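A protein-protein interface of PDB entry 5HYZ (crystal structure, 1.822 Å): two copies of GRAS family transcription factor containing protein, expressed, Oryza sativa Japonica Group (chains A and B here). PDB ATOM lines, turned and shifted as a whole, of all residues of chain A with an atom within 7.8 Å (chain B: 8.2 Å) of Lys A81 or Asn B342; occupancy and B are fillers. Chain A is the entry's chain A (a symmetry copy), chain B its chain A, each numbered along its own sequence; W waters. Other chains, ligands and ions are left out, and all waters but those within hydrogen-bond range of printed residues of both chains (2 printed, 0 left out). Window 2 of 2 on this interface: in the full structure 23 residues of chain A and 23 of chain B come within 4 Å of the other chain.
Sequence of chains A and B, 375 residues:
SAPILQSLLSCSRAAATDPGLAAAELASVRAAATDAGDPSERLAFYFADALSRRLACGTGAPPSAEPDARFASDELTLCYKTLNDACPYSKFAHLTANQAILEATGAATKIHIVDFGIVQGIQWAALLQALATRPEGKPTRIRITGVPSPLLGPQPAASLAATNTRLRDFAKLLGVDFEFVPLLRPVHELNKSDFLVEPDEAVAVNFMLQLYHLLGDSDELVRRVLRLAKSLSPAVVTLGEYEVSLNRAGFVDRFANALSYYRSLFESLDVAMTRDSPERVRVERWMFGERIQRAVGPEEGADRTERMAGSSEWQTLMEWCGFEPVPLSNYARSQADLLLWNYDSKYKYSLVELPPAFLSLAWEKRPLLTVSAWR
O of Asn B342 lies within hydrogen-bond range of NZ of Lys A81 (2.5 Å). The guanidinium group (NH2) of Arg A166 sits at hydrogen-bond distance from the backbone carbonyl oxygen (O) of Trp B341, at 2.7 Å.
Among the printed residues, merely in contact across the chains: Ile A122 with Asn B342 (3.4 Å) and Ile A122 with Trp B341 (3.5 Å).
Lys A81 touches just one residue of chain B: Asn B342 (2.5 Å). Of the printed residues of chain B, Ile A122 touches Trp B341 (3.5 Å) and Asn B342 (3.4 Å). Of the printed residues of chain B, Arg A166 touches Trp B341 (2.7 Å). Of the printed residues of chain A, Trp B341 touches Ile A122 and Arg A166. Of the printed residues of chain A, Asn B342 touches Lys A81 and Ile A122. The nearest residue of chain B that does not touch Lys A81 is Asp B344 (4.4 Å). The nearest residue of chain A that does not touch Asn B342 is Arg A166 (4.7 Å).
Of the 25 printed residues of chain A, 3 touch a printed residue of chain B. Of the 12 printed residues of chain B, 2 touch a printed residue of chain A. Hydrophobic or aromatic side chains of chain B that line the printed part of chain A: Trp B341. Among the printed residues, 4 pairs touch across the chains. Among the printed residues, no Asp or Glu carboxylate lies within 4 Å of a Lys or Arg side-chain nitrogen of the other chain.
No position is printed for both chains.
Water W2 bridges the backbone carbonyl oxygen (O) of Trp B341 (2.7 Å) and the guanidinium group (NH1) of Arg A166 (3.3 Å). Water W1 lies within hydrogen-bond range of O of Asp B337 (2.8 Å) and NH2 of Arg A166 (3.2 Å).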
ATOM      1  N   GLU A  75      22.036 -15.829  -6.652  1.00  0.00           N
ATOM      2  CA  GLU A  75      21.296 -15.788  -5.405  1.00  0.00           C
ATOM      3  C   GLU A  75      22.157 -15.138  -4.354  1.00  0.00           C
ATOM      4  O   GLU A  75      21.807 -14.080  -3.865  1.00  0.00           O
ATOM      5  CB  GLU A  75      20.846 -17.187  -4.981  1.00  0.00           C
ATOM      6  CG  GLU A  75      19.816 -17.815  -5.925  1.00  0.00           C
ATOM      7  CD  GLU A  75      18.586 -16.927  -6.159  1.00  0.00           C
ATOM      8  OE1 GLU A  75      17.493 -17.292  -5.688  1.00  0.00           O
ATOM      9  OE2 GLU A  75      18.690 -15.874  -6.827  1.00  0.00           O
ATOM     10  N   LEU A  76      23.310 -15.735  -4.073  1.00  0.00           N
ATOM     11  CA  LEU A  76      24.212 -15.218  -3.052  1.00  0.00           C
ATOM     12  C   LEU A  76      24.593 -13.749  -3.214  1.00  0.00           C
ATOM     13  O   LEU A  76      24.665 -13.028  -2.235  1.00  0.00           O
ATOM     14  CB  LEU A  76      25.489 -16.043  -3.012  1.00  0.00           C
ATOM     15  CG  LEU A  76      25.323 -17.399  -2.361  1.00  0.00           C
ATOM     16  CD1 LEU A  76      26.709 -17.978  -2.153  1.00  0.00           C
ATOM     17  CD2 LEU A  76      24.558 -17.257  -1.044  1.00  0.00           C
ATOM     18  N   THR A  77      24.854 -13.304  -4.433  1.00  0.00           N
ATOM     19  CA  THR A  77      25.350 -11.950  -4.581  1.00  0.00           C
ATOM     20  C   THR A  77      24.190 -10.972  -4.261  1.00  0.00           C
ATOM     21  O   THR A  77      24.384  -9.952  -3.549  1.00  0.00           O
ATOM     22  CB  THR A  77      25.971 -11.741  -5.994  1.00  0.00           C
ATOM     23  OG1 THR A  77      26.762 -10.547  -6.005  1.00  0.00           O
ATOM     24  CG2 THR A  77      24.904 -11.702  -7.085  1.00  0.00           C
ATOM     25  N   LEU A  78      22.984 -11.327  -4.700  1.00  0.00           N
ATOM     26  CA  LEU A  78      21.813 -10.528  -4.367  1.00  0.00           C
ATOM     27  C   LEU A  78      21.535 -10.534  -2.875  1.00  0.00           C
ATOM     28  O   LEU A  78      21.127  -9.512  -2.298  1.00  0.00           O
ATOM     29  CB  LEU A  78      20.581 -11.046  -5.100  1.00  0.00           C
ATOM     30  CG  LEU A  78      20.216 -10.359  -6.420  1.00  0.00           C
ATOM     31  CD1 LEU A  78      21.458 -10.067  -7.266  1.00  0.00           C
ATOM     32  CD2 LEU A  78      19.255 -11.276  -7.151  1.00  0.00           C
ATOM     33  N   CYS A  79      21.734 -11.709  -2.273  1.00  0.00           N
ATOM     34  CA  CYS A  79      21.508 -11.918  -0.841  1.00  0.00           C
ATOM     35  C   CYS A  79      22.432 -11.057  -0.034  1.00  0.00           C
ATOM     36  O   CYS A  79      22.006 -10.420   0.898  1.00  0.00           O
ATOM     37  CB  CYS A  79      21.740 -13.380  -0.450  1.00  0.00           C
ATOM     38  SG  CYS A  79      20.438 -14.493  -1.004  1.00  0.00           S
ATOM     39  N   TYR A  80      23.711 -11.109  -0.378  1.00  0.00           N
ATOM     40  CA  TYR A  80      24.741 -10.310   0.257  1.00  0.00           C
ATOM     41  C   TYR A  80      24.358  -8.846   0.225  1.00  0.00           C
ATOM     42  O   TYR A  80      24.444  -8.145   1.252  1.00  0.00           O
ATOM     43  CB  TYR A  80      26.096 -10.536  -0.431  1.00  0.00           C
ATOM     44  CG  TYR A  80      27.249  -9.784   0.190  1.00  0.00           C
ATOM     45  CD1 TYR A  80      27.837 -10.230   1.374  1.00  0.00           C
ATOM     46  CD2 TYR A  80      27.768  -8.636  -0.419  1.00  0.00           C
ATOM     47  CE1 TYR A  80      28.918  -9.553   1.950  1.00  0.00           C
ATOM     48  CE2 TYR A  80      28.853  -7.941   0.152  1.00  0.00           C
ATOM     49  CZ  TYR A  80      29.422  -8.414   1.335  1.00  0.00           C
ATOM     50  OH  TYR A  80      30.487  -7.711   1.911  1.00  0.00           O
ATOM     51  N   LYS A  81      23.925  -8.374  -0.941  1.00  0.00           N
ATOM     52  CA  LYS A  81      23.528  -6.958  -1.060  1.00  0.00           C
ATOM     53  C   LYS A  81      22.295  -6.598  -0.181  1.00  0.00           C
ATOM     54  O   LYS A  81      22.270  -5.585   0.529  1.00  0.00           O
ATOM     55  CB  LYS A  81      23.273  -6.635  -2.548  1.00  0.00           C
ATOM     56  CG  LYS A  81      22.778  -5.217  -2.833  1.00  0.00           C
ATOM     57  CD  LYS A  81      23.945  -4.227  -2.860  1.00  0.00           C
ATOM     58  CE  LYS A  81      23.508  -2.777  -3.174  1.00  0.00           C
ATOM     59  NZ  LYS A  81      24.710  -1.911  -3.469  1.00  0.00           N
ATOM     60  N   THR A  82      21.266  -7.439  -0.242  1.00  0.00           N
ATOM     61  CA  THR A  82      20.109  -7.280   0.609  1.00  0.00           C
ATOM     62  C   THR A  82      20.490  -7.235   2.117  1.00  0.00           C
ATOM     63  O   THR A  82      20.045  -6.333   2.858  1.00  0.00           O
ATOM     64  CB  THR A  82      19.123  -8.439   0.376  1.00  0.00           C
ATOM     65  OG1 THR A  82      18.552  -8.277  -0.918  1.00  0.00           O
ATOM     66  CG2 THR A  82      18.019  -8.401   1.351  1.00  0.00           C
ATOM     67  N   LEU A  83      21.285  -8.230   2.541  1.00  0.00           N
ATOM     68  CA  LEU A  83      21.640  -8.371   3.953  1.00  0.00           C
ATOM     69  C   LEU A  83      22.344  -7.110   4.377  1.00  0.00           C
ATOM     70  O   LEU A  83      22.052  -6.575   5.435  1.00  0.00           O
ATOM     71  CB  LEU A  83      22.512  -9.607   4.186  1.00  0.00           C
ATOM     72  CG  LEU A  83      22.912 -10.004   5.612  1.00  0.00           C
ATOM     73  CD1 LEU A  83      21.686 -10.159   6.529  1.00  0.00           C
ATOM     74  CD2 LEU A  83      23.739 -11.262   5.606  1.00  0.00           C
ATOM     75  N   ASN A  84      23.258  -6.613   3.543  1.00  0.00           N
ATOM     76  CA  ASN A  84      24.047  -5.460   3.953  1.00  0.00           C
ATOM     77  C   ASN A  84      23.337  -4.122   3.831  1.00  0.00           C
ATOM     78  O   ASN A  84      23.723  -3.145   4.494  1.00  0.00           O
ATOM     79  CB  ASN A  84      25.354  -5.438   3.180  1.00  0.00           C
ATOM     80  CG  ASN A  84      26.179  -6.727   3.397  1.00  0.00           C
ATOM     81  OD1 ASN A  84      26.123  -7.378   4.454  1.00  0.00           O
ATOM     82  ND2 ASN A  84      26.935  -7.104   2.371  1.00  0.00           N
ATOM     83  N   ASP A  85      22.277  -4.069   3.034  1.00  0.00           N
ATOM     84  CA  ASP A  85      21.397  -2.921   3.113  1.00  0.00           C
ATOM     85  C   ASP A  85      20.481  -2.974   4.381  1.00  0.00           C
ATOM     86  O   ASP A  85      20.114  -1.961   4.947  1.00  0.00           O
ATOM     87  CB  ASP A  85      20.559  -2.814   1.836  1.00  0.00           C
ATOM     88  CG  ASP A  85      19.698  -1.573   1.832  1.00  0.00           C
ATOM     89  OD1 ASP A  85      20.224  -0.484   1.518  1.00  0.00           O
ATOM     90  OD2 ASP A  85      18.501  -1.678   2.178  1.00  0.00           O
ATOM     91  N   ALA A  86      20.146  -4.160   4.857  1.00  0.00           N
ATOM     92  CA  ALA A  86      19.226  -4.235   5.989  1.00  0.00           C
ATOM     93  C   ALA A  86      19.905  -4.239   7.351  1.00  0.00           C
ATOM     94  O   ALA A  86      19.285  -3.927   8.373  1.00  0.00           O
ATOM     95  CB  ALA A  86      18.365  -5.498   5.853  1.00  0.00           C
ATOM     96  N   CYS A  87      21.158  -4.668   7.383  1.00  0.00           N
ATOM     97  CA  CYS A  87      21.841  -4.966   8.631  1.00  0.00           C
ATOM     98  C   CYS A  87      23.242  -4.352   8.607  1.00  0.00           C
ATOM     99  O   CYS A  87      23.794  -4.126   7.531  1.00  0.00           O
ATOM    100  CB  CYS A  87      21.968  -6.471   8.813  1.00  0.00           C
ATOM    101  SG  CYS A  87      20.341  -7.339   8.855  1.00  0.00           S
ATOM    102  N   SER A  90      28.242  -6.254   7.640  1.00  0.00           N
ATOM    103  CA  SER A  90      29.436  -6.088   6.832  1.00  0.00           C
ATOM    104  C   SER A  90      30.109  -4.744   7.109  1.00  0.00           C
ATOM    105  O   SER A  90      31.334  -4.653   7.120  1.00  0.00           O
ATOM    106  CB  SER A  90      29.138  -6.255   5.309  1.00  0.00           C
ATOM    107  OG  SER A  90      28.293  -5.193   4.853  1.00  0.00           O
ATOM    108  N   LYS A  91      29.341  -3.696   7.380  1.00  0.00           N
ATOM    109  CA  LYS A  91      29.955  -2.430   7.625  1.00  0.00           C
ATOM    110  C   LYS A  91      30.745  -2.484   8.934  1.00  0.00           C
ATOM    111  O   LYS A  91      31.851  -1.940   9.034  1.00  0.00           O
ATOM    112  CB  LYS A  91      28.885  -1.294   7.654  1.00  0.00           C
ATOM    113  CG  LYS A  91      29.527   0.102   7.646  1.00  0.00           C
ATOM    114  CD  LYS A  91      28.624   1.200   7.055  1.00  0.00           C
ATOM    115  CE  LYS A  91      29.378   2.542   6.875  1.00  0.00           C
ATOM    116  NZ  LYS A  91      28.598   3.763   7.349  1.00  0.00           N
ATOM    117  N   HIS A  94      34.013  -4.474   8.212  1.00  0.00           N
ATOM    118  CA  HIS A  94      34.978  -3.666   7.422  1.00  0.00           C
ATOM    119  C   HIS A  94      35.583  -2.495   8.141  1.00  0.00           C
ATOM    120  O   HIS A  94      36.767  -2.246   8.058  1.00  0.00           O
ATOM    121  CB  HIS A  94      34.274  -3.087   6.166  1.00  0.00           C
ATOM    122  CG  HIS A  94      33.836  -4.141   5.227  1.00  0.00           C
ATOM    123  ND1 HIS A  94      32.918  -3.906   4.212  1.00  0.00           N
ATOM    124  CD2 HIS A  94      34.188  -5.449   5.134  1.00  0.00           C
ATOM    125  CE1 HIS A  94      32.732  -5.030   3.537  1.00  0.00           C
ATOM    126  NE2 HIS A  94      33.495  -5.975   4.070  1.00  0.00           N
ATOM    127  N   VAL A 119      34.806  -9.129  -2.104  1.00  0.00           N
ATOM    128  CA  VAL A 119      33.500  -9.210  -2.771  1.00  0.00           C
ATOM    129  C   VAL A 119      33.356  -7.991  -3.704  1.00  0.00           C
ATOM    130  O   VAL A 119      33.463  -8.112  -4.892  1.00  0.00           O
ATOM    131  CB  VAL A 119      32.312  -9.269  -1.719  1.00  0.00           C
ATOM    132  CG1 VAL A 119      30.981  -9.344  -2.474  1.00  0.00           C
ATOM    133  CG2 VAL A 119      32.527 -10.511  -0.825  1.00  0.00           C
ATOM    134  N   GLN A 120      33.184  -6.812  -3.150  1.00  0.00           N
ATOM    135  CA  GLN A 120      33.059  -5.572  -3.917  1.00  0.00           C
ATOM    136  C   GLN A 120      34.155  -4.650  -3.335  1.00  0.00           C
ATOM    137  O   GLN A 120      34.945  -4.995  -2.463  1.00  0.00           O
ATOM    138  CB  GLN A 120      31.691  -4.890  -3.783  1.00  0.00           C
ATOM    139  CG  GLN A 120      30.473  -5.514  -4.523  1.00  0.00           C
ATOM    140  CD  GLN A 120      30.676  -5.842  -6.023  1.00  0.00           C
ATOM    141  OE1 GLN A 120      31.052  -6.955  -6.371  1.00  0.00           O
ATOM    142  NE2 GLN A 120      30.359  -4.894  -6.898  1.00  0.00           N
ATOM    143  N   GLY A 121      34.232  -3.466  -3.831  1.00  0.00           N
ATOM    144  CA  GLY A 121      35.406  -2.767  -3.319  1.00  0.00           C
ATOM    145  C   GLY A 121      35.225  -1.915  -2.071  1.00  0.00           C
ATOM    146  O   GLY A 121      36.145  -1.224  -1.672  1.00  0.00           O
ATOM    147  N   ILE A 122      34.058  -1.960  -1.451  1.00  0.00           N
ATOM    148  CA  ILE A 122      33.759  -0.832  -0.519  1.00  0.00           C
ATOM    149  C   ILE A 122      34.675  -0.797   0.704  1.00  0.00           C
ATOM    150  O   ILE A 122      35.040   0.296   1.166  1.00  0.00           O
ATOM    151  CB  ILE A 122      32.266  -0.857  -0.112  1.00  0.00           C
ATOM    152  CG1 ILE A 122      31.913   0.525   0.517  1.00  0.00           C
ATOM    153  CG2 ILE A 122      32.009  -1.998   0.810  1.00  0.00           C
ATOM    154  CD1 ILE A 122      30.413   0.758   0.794  1.00  0.00           C
ATOM    155  N   GLN A 123      35.120  -1.975   1.209  1.00  0.00           N
ATOM    156  CA  GLN A 123      36.069  -1.907   2.326  1.00  0.00           C
ATOM    157  C   GLN A 123      37.299  -1.083   1.955  1.00  0.00           C
ATOM    158  O   GLN A 123      37.848  -0.307   2.738  1.00  0.00           O
ATOM    159  CB  GLN A 123      36.525  -3.341   2.739  1.00  0.00           C
ATOM    160  CG  GLN A 123      37.497  -3.278   3.979  1.00  0.00           C
ATOM    161  CD  GLN A 123      37.834  -4.678   4.591  1.00  0.00           C
ATOM    162  OE1 GLN A 123      37.416  -5.741   4.079  1.00  0.00           O
ATOM    163  NE2 GLN A 123      38.619  -4.656   5.638  1.00  0.00           N
ATOM    164  N   LEU A 151      31.524 -15.884  -2.784  1.00  0.00           N
ATOM    165  CA  LEU A 151      30.252 -15.190  -3.079  1.00  0.00           C
ATOM    166  C   LEU A 151      30.185 -14.695  -4.529  1.00  0.00           C
ATOM    167  O   LEU A 151      29.095 -14.580  -5.102  1.00  0.00           O
ATOM    168  CB  LEU A 151      30.033 -14.013  -2.155  1.00  0.00           C
ATOM    169  CG  LEU A 151      29.622 -14.242  -0.696  1.00  0.00           C
ATOM    170  CD1 LEU A 151      30.056 -13.101   0.186  1.00  0.00           C
ATOM    171  CD2 LEU A 151      28.119 -14.442  -0.581  1.00  0.00           C
ATOM    172  N   ARG A 166      36.662   0.715 -10.466  1.00  0.00           N
ATOM    173  CA  ARG A 166      36.064   1.635  -9.512  1.00  0.00           C
ATOM    174  C   ARG A 166      37.056   2.104  -8.444  1.00  0.00           C
ATOM    175  O   ARG A 166      37.093   3.294  -8.095  1.00  0.00           O
ATOM    176  CB  ARG A 166      34.847   0.945  -8.897  1.00  0.00           C
ATOM    177  CG  ARG A 166      33.717   1.842  -8.689  1.00  0.00           C
ATOM    178  CD  ARG A 166      32.476   1.124  -8.125  1.00  0.00           C
ATOM    179  NE  ARG A 166      31.633   2.168  -7.552  1.00  0.00           N
ATOM    180  CZ  ARG A 166      30.557   1.943  -6.812  1.00  0.00           C
ATOM    181  NH1 ARG A 166      30.205   0.703  -6.540  1.00  0.00           N
ATOM    182  NH2 ARG A 166      29.866   2.961  -6.347  1.00  0.00           N
ATOM    183  N   VAL A 283      17.099 -14.195   1.093  1.00  0.00           N
ATOM    184  CA  VAL A 283      18.193 -14.328   2.053  1.00  0.00           C
ATOM    185  C   VAL A 283      17.984 -15.540   2.966  1.00  0.00           C
ATOM    186  O   VAL A 283      18.888 -16.370   3.149  1.00  0.00           O
ATOM    187  CB  VAL A 283      18.316 -13.053   2.921  1.00  0.00           C
ATOM    188  CG1 VAL A 283      19.326 -13.283   4.082  1.00  0.00           C
ATOM    189  CG2 VAL A 283      18.753 -11.887   2.031  1.00  0.00           C
ATOM    190  N   MET A 287      20.601 -18.136   1.355  1.00  0.00           N
ATOM    191  CA  MET A 287      21.846 -17.931   2.084  1.00  0.00           C
ATOM    192  C   MET A 287      21.758 -18.690   3.408  1.00  0.00           C
ATOM    193  O   MET A 287      22.473 -19.674   3.579  1.00  0.00           O
ATOM    194  CB  MET A 287      22.129 -16.446   2.303  1.00  0.00           C
ATOM    195  CG  MET A 287      23.464 -16.225   2.987  1.00  0.00           C
ATOM    196  SD  MET A 287      23.812 -14.272   3.125  1.00  0.00           S
ATOM    197  CE  MET A 287      25.010 -14.078   1.531  1.00  0.00           C
ATOM    198  N   ALA B 336      32.297  12.061  -0.524  1.00  0.00           N
ATOM    199  CA  ALA B 336      30.932  11.946  -1.059  1.00  0.00           C
ATOM    200  C   ALA B 336      30.732  10.776  -2.013  1.00  0.00           C
ATOM    201  O   ALA B 336      29.699  10.121  -1.959  1.00  0.00           O
ATOM    202  CB  ALA B 336      30.527  13.299  -1.728  1.00  0.00           C
ATOM    203  N   ASP B 337      31.731  10.435  -2.848  1.00  0.00           N
ATOM    204  CA  ASP B 337      31.680   9.193  -3.611  1.00  0.00           C
ATOM    205  C   ASP B 337      31.664   7.963  -2.769  1.00  0.00           C
ATOM    206  O   ASP B 337      30.984   6.999  -3.068  1.00  0.00           O
ATOM    207  CB  ASP B 337      32.870   9.123  -4.562  1.00  0.00           C
ATOM    208  CG  ASP B 337      32.503   9.533  -5.972  1.00  0.00           C
ATOM    209  OD1 ASP B 337      31.325   9.904  -6.220  1.00  0.00           O
ATOM    210  OD2 ASP B 337      33.391   9.485  -6.847  1.00  0.00           O
ATOM    211  N   LEU B 338      32.392   7.991  -1.660  1.00  0.00           N
ATOM    212  CA  LEU B 338      32.392   6.852  -0.781  1.00  0.00           C
ATOM    213  C   LEU B 338      30.995   6.652  -0.224  1.00  0.00           C
ATOM    214  O   LEU B 338      30.476   5.538  -0.127  1.00  0.00           O
ATOM    215  CB  LEU B 338      33.410   7.060   0.348  1.00  0.00           C
ATOM    216  CG  LEU B 338      33.423   6.005   1.436  1.00  0.00           C
ATOM    217  CD1 LEU B 338      33.589   4.581   0.862  1.00  0.00           C
ATOM    218  CD2 LEU B 338      34.479   6.266   2.530  1.00  0.00           C
ATOM    219  N   LEU B 339      30.342   7.754   0.155  1.00  0.00           N
ATOM    220  CA  LEU B 339      29.029   7.623   0.747  1.00  0.00           C
ATOM    221  C   LEU B 339      28.068   7.002  -0.272  1.00  0.00           C
ATOM    222  O   LEU B 339      27.184   6.230   0.076  1.00  0.00           O
ATOM    223  CB  LEU B 339      28.568   9.045   1.200  1.00  0.00           C
ATOM    224  CG  LEU B 339      27.060   9.114   1.198  1.00  0.00           C
ATOM    225  CD1 LEU B 339      26.597   8.364   2.443  1.00  0.00           C
ATOM    226  CD2 LEU B 339      26.604  10.559   1.153  1.00  0.00           C
ATOM    227  N   LEU B 340      28.289   7.276  -1.553  1.00  0.00           N
ATOM    228  CA  LEU B 340      27.351   6.841  -2.576  1.00  0.00           C
ATOM    229  C   LEU B 340      27.681   5.435  -3.108  1.00  0.00           C
ATOM    230  O   LEU B 340      26.991   4.916  -3.997  1.00  0.00           O
ATOM    231  CB  LEU B 340      27.351   7.846  -3.750  1.00  0.00           C
ATOM    232  CG  LEU B 340      26.793   9.259  -3.451  1.00  0.00           C
ATOM    233  CD1 LEU B 340      26.953  10.177  -4.660  1.00  0.00           C
ATOM    234  CD2 LEU B 340      25.314   9.166  -3.002  1.00  0.00           C
ATOM    235  N   TRP B 341      28.749   4.840  -2.584  1.00  0.00           N
ATOM    236  CA  TRP B 341      29.302   3.623  -3.193  1.00  0.00           C
ATOM    237  C   TRP B 341      28.282   2.522  -3.367  1.00  0.00           C
ATOM    238  O   TRP B 341      28.256   1.862  -4.412  1.00  0.00           O
ATOM    239  CB  TRP B 341      30.465   3.087  -2.352  1.00  0.00           C
ATOM    240  CG  TRP B 341      31.339   2.069  -3.033  1.00  0.00           C
ATOM    241  CD1 TRP B 341      31.156   0.721  -3.050  1.00  0.00           C
ATOM    242  CD2 TRP B 341      32.591   2.321  -3.730  1.00  0.00           C
ATOM    243  NE1 TRP B 341      32.199   0.118  -3.739  1.00  0.00           N
ATOM    244  CE2 TRP B 341      33.101   1.070  -4.133  1.00  0.00           C
ATOM    245  CE3 TRP B 341      33.307   3.473  -4.037  1.00  0.00           C
ATOM    246  CZ2 TRP B 341      34.300   0.936  -4.840  1.00  0.00           C
ATOM    247  CZ3 TRP B 341      34.504   3.336  -4.740  1.00  0.00           C
ATOM    248  CH2 TRP B 341      34.972   2.099  -5.140  1.00  0.00           C
ATOM    249  N   ASN B 342      27.443   2.302  -2.365  1.00  0.00           N
ATOM    250  CA  ASN B 342      26.481   1.194  -2.480  1.00  0.00           C
ATOM    251  C   ASN B 342      25.155   1.469  -3.207  1.00  0.00           C
ATOM    252  O   ASN B 342      24.328   0.554  -3.376  1.00  0.00           O
ATOM    253  CB  ASN B 342      26.153   0.653  -1.084  1.00  0.00           C
ATOM    254  CG  ASN B 342      27.168  -0.363  -0.620  1.00  0.00           C
ATOM    255  OD1 ASN B 342      27.878  -0.973  -1.446  1.00  0.00           O
ATOM    256  ND2 ASN B 342      27.266  -0.549   0.703  1.00  0.00           N
ATOM    257  N   TYR B 343      24.923   2.714  -3.603  1.00  0.00           N
ATOM    258  CA  TYR B 343      23.789   3.000  -4.475  1.00  0.00           C
ATOM    259  C   TYR B 343      24.041   2.423  -5.878  1.00  0.00           C
ATOM    260  O   TYR B 343      24.817   2.994  -6.660  1.00  0.00           O
ATOM    261  CB  TYR B 343      23.521   4.508  -4.524  1.00  0.00           C
ATOM    262  CG  TYR B 343      22.978   5.014  -3.194  1.00  0.00           C
ATOM    263  CD1 TYR B 343      21.619   4.882  -2.890  1.00  0.00           C
ATOM    264  CD2 TYR B 343      23.822   5.565  -2.229  1.00  0.00           C
ATOM    265  CE1 TYR B 343      21.112   5.333  -1.677  1.00  0.00           C
ATOM    266  CE2 TYR B 343      23.342   5.967  -1.013  1.00  0.00           C
ATOM    267  CZ  TYR B 343      21.982   5.857  -0.752  1.00  0.00           C
ATOM    268  OH  TYR B 343      21.492   6.277   0.433  1.00  0.00           O
ATOM    269  N   ASP B 344      23.366   1.304  -6.172  1.00  0.00           N
ATOM    270  CA  ASP B 344      23.503   0.589  -7.448  1.00  0.00           C
ATOM    271  C   ASP B 344      23.047   1.412  -8.640  1.00  0.00           C
ATOM    272  O   ASP B 344      22.694   2.596  -8.513  1.00  0.00           O
ATOM    273  CB  ASP B 344      22.717  -0.733  -7.421  1.00  0.00           C
ATOM    274  CG  ASP B 344      21.224  -0.541  -7.671  1.00  0.00           C
ATOM    275  OD1 ASP B 344      20.659   0.490  -7.252  1.00  0.00           O
ATOM    276  OD2 ASP B 344      20.605  -1.426  -8.296  1.00  0.00           O
ATOM    277  N   SER B 345      23.019   0.763  -9.800  1.00  0.00           N
ATOM    278  CA  SER B 345      22.855   1.488 -11.052  1.00  0.00           C
ATOM    279  C   SER B 345      21.494   2.168 -11.212  1.00  0.00           C
ATOM    280  O   SER B 345      21.375   3.143 -11.975  1.00  0.00           O
ATOM    281  CB  SER B 345      23.103   0.536 -12.258  1.00  0.00           C
ATOM    282  OG  SER B 345      21.973  -0.311 -12.519  1.00  0.00           O
ATOM    283  N   LYS B 346      20.449   1.688 -10.531  1.00  0.00           N
ATOM    284  CA  LYS B 346      19.149   2.336 -10.713  1.00  0.00           C
ATOM    285  C   LYS B 346      19.091   3.708 -10.028  1.00  0.00           C
ATOM    286  O   LYS B 346      18.228   4.531 -10.358  1.00  0.00           O
ATOM    287  CB  LYS B 346      18.005   1.453 -10.216  1.00  0.00           C
ATOM    288  CG  LYS B 346      18.045   1.096  -8.746  1.00  0.00           C
ATOM    289  CD  LYS B 346      17.017  -0.023  -8.438  1.00  0.00           C
ATOM    290  CE  LYS B 346      16.684  -0.146  -6.949  1.00  0.00           C
ATOM    291  NZ  LYS B 346      17.774  -0.826  -6.181  1.00  0.00           N
ATOM    292  N   TYR B 347      20.007   3.965  -9.101  1.00  0.00           N
ATOM    293  CA  TYR B 347      20.068   5.303  -8.480  1.00  0.00           C
ATOM    294  C   TYR B 347      20.796   6.275  -9.383  1.00  0.00           C
ATOM    295  O   TYR B 347      21.660   5.880 -10.151  1.00  0.00           O
ATOM    296  CB  TYR B 347      20.740   5.225  -7.115  1.00  0.00           C
ATOM    297  CG  TYR B 347      19.920   4.487  -6.085  1.00  0.00           C
ATOM    298  CD1 TYR B 347      18.955   5.146  -5.359  1.00  0.00           C
ATOM    299  CD2 TYR B 347      20.125   3.129  -5.830  1.00  0.00           C
ATOM    300  CE1 TYR B 347      18.208   4.471  -4.383  1.00  0.00           C
ATOM    301  CE2 TYR B 347      19.379   2.446  -4.874  1.00  0.00           C
ATOM    302  CZ  TYR B 347      18.435   3.135  -4.151  1.00  0.00           C
ATOM    303  OH  TYR B 347      17.691   2.519  -3.178  1.00  0.00           O
HETATM  304  O   HOH W   1      30.394   6.032  -5.644  1.00  0.00           O
HETATM  305  O   HOH W   2      26.927   0.205  -6.148  1.00  0.00           O
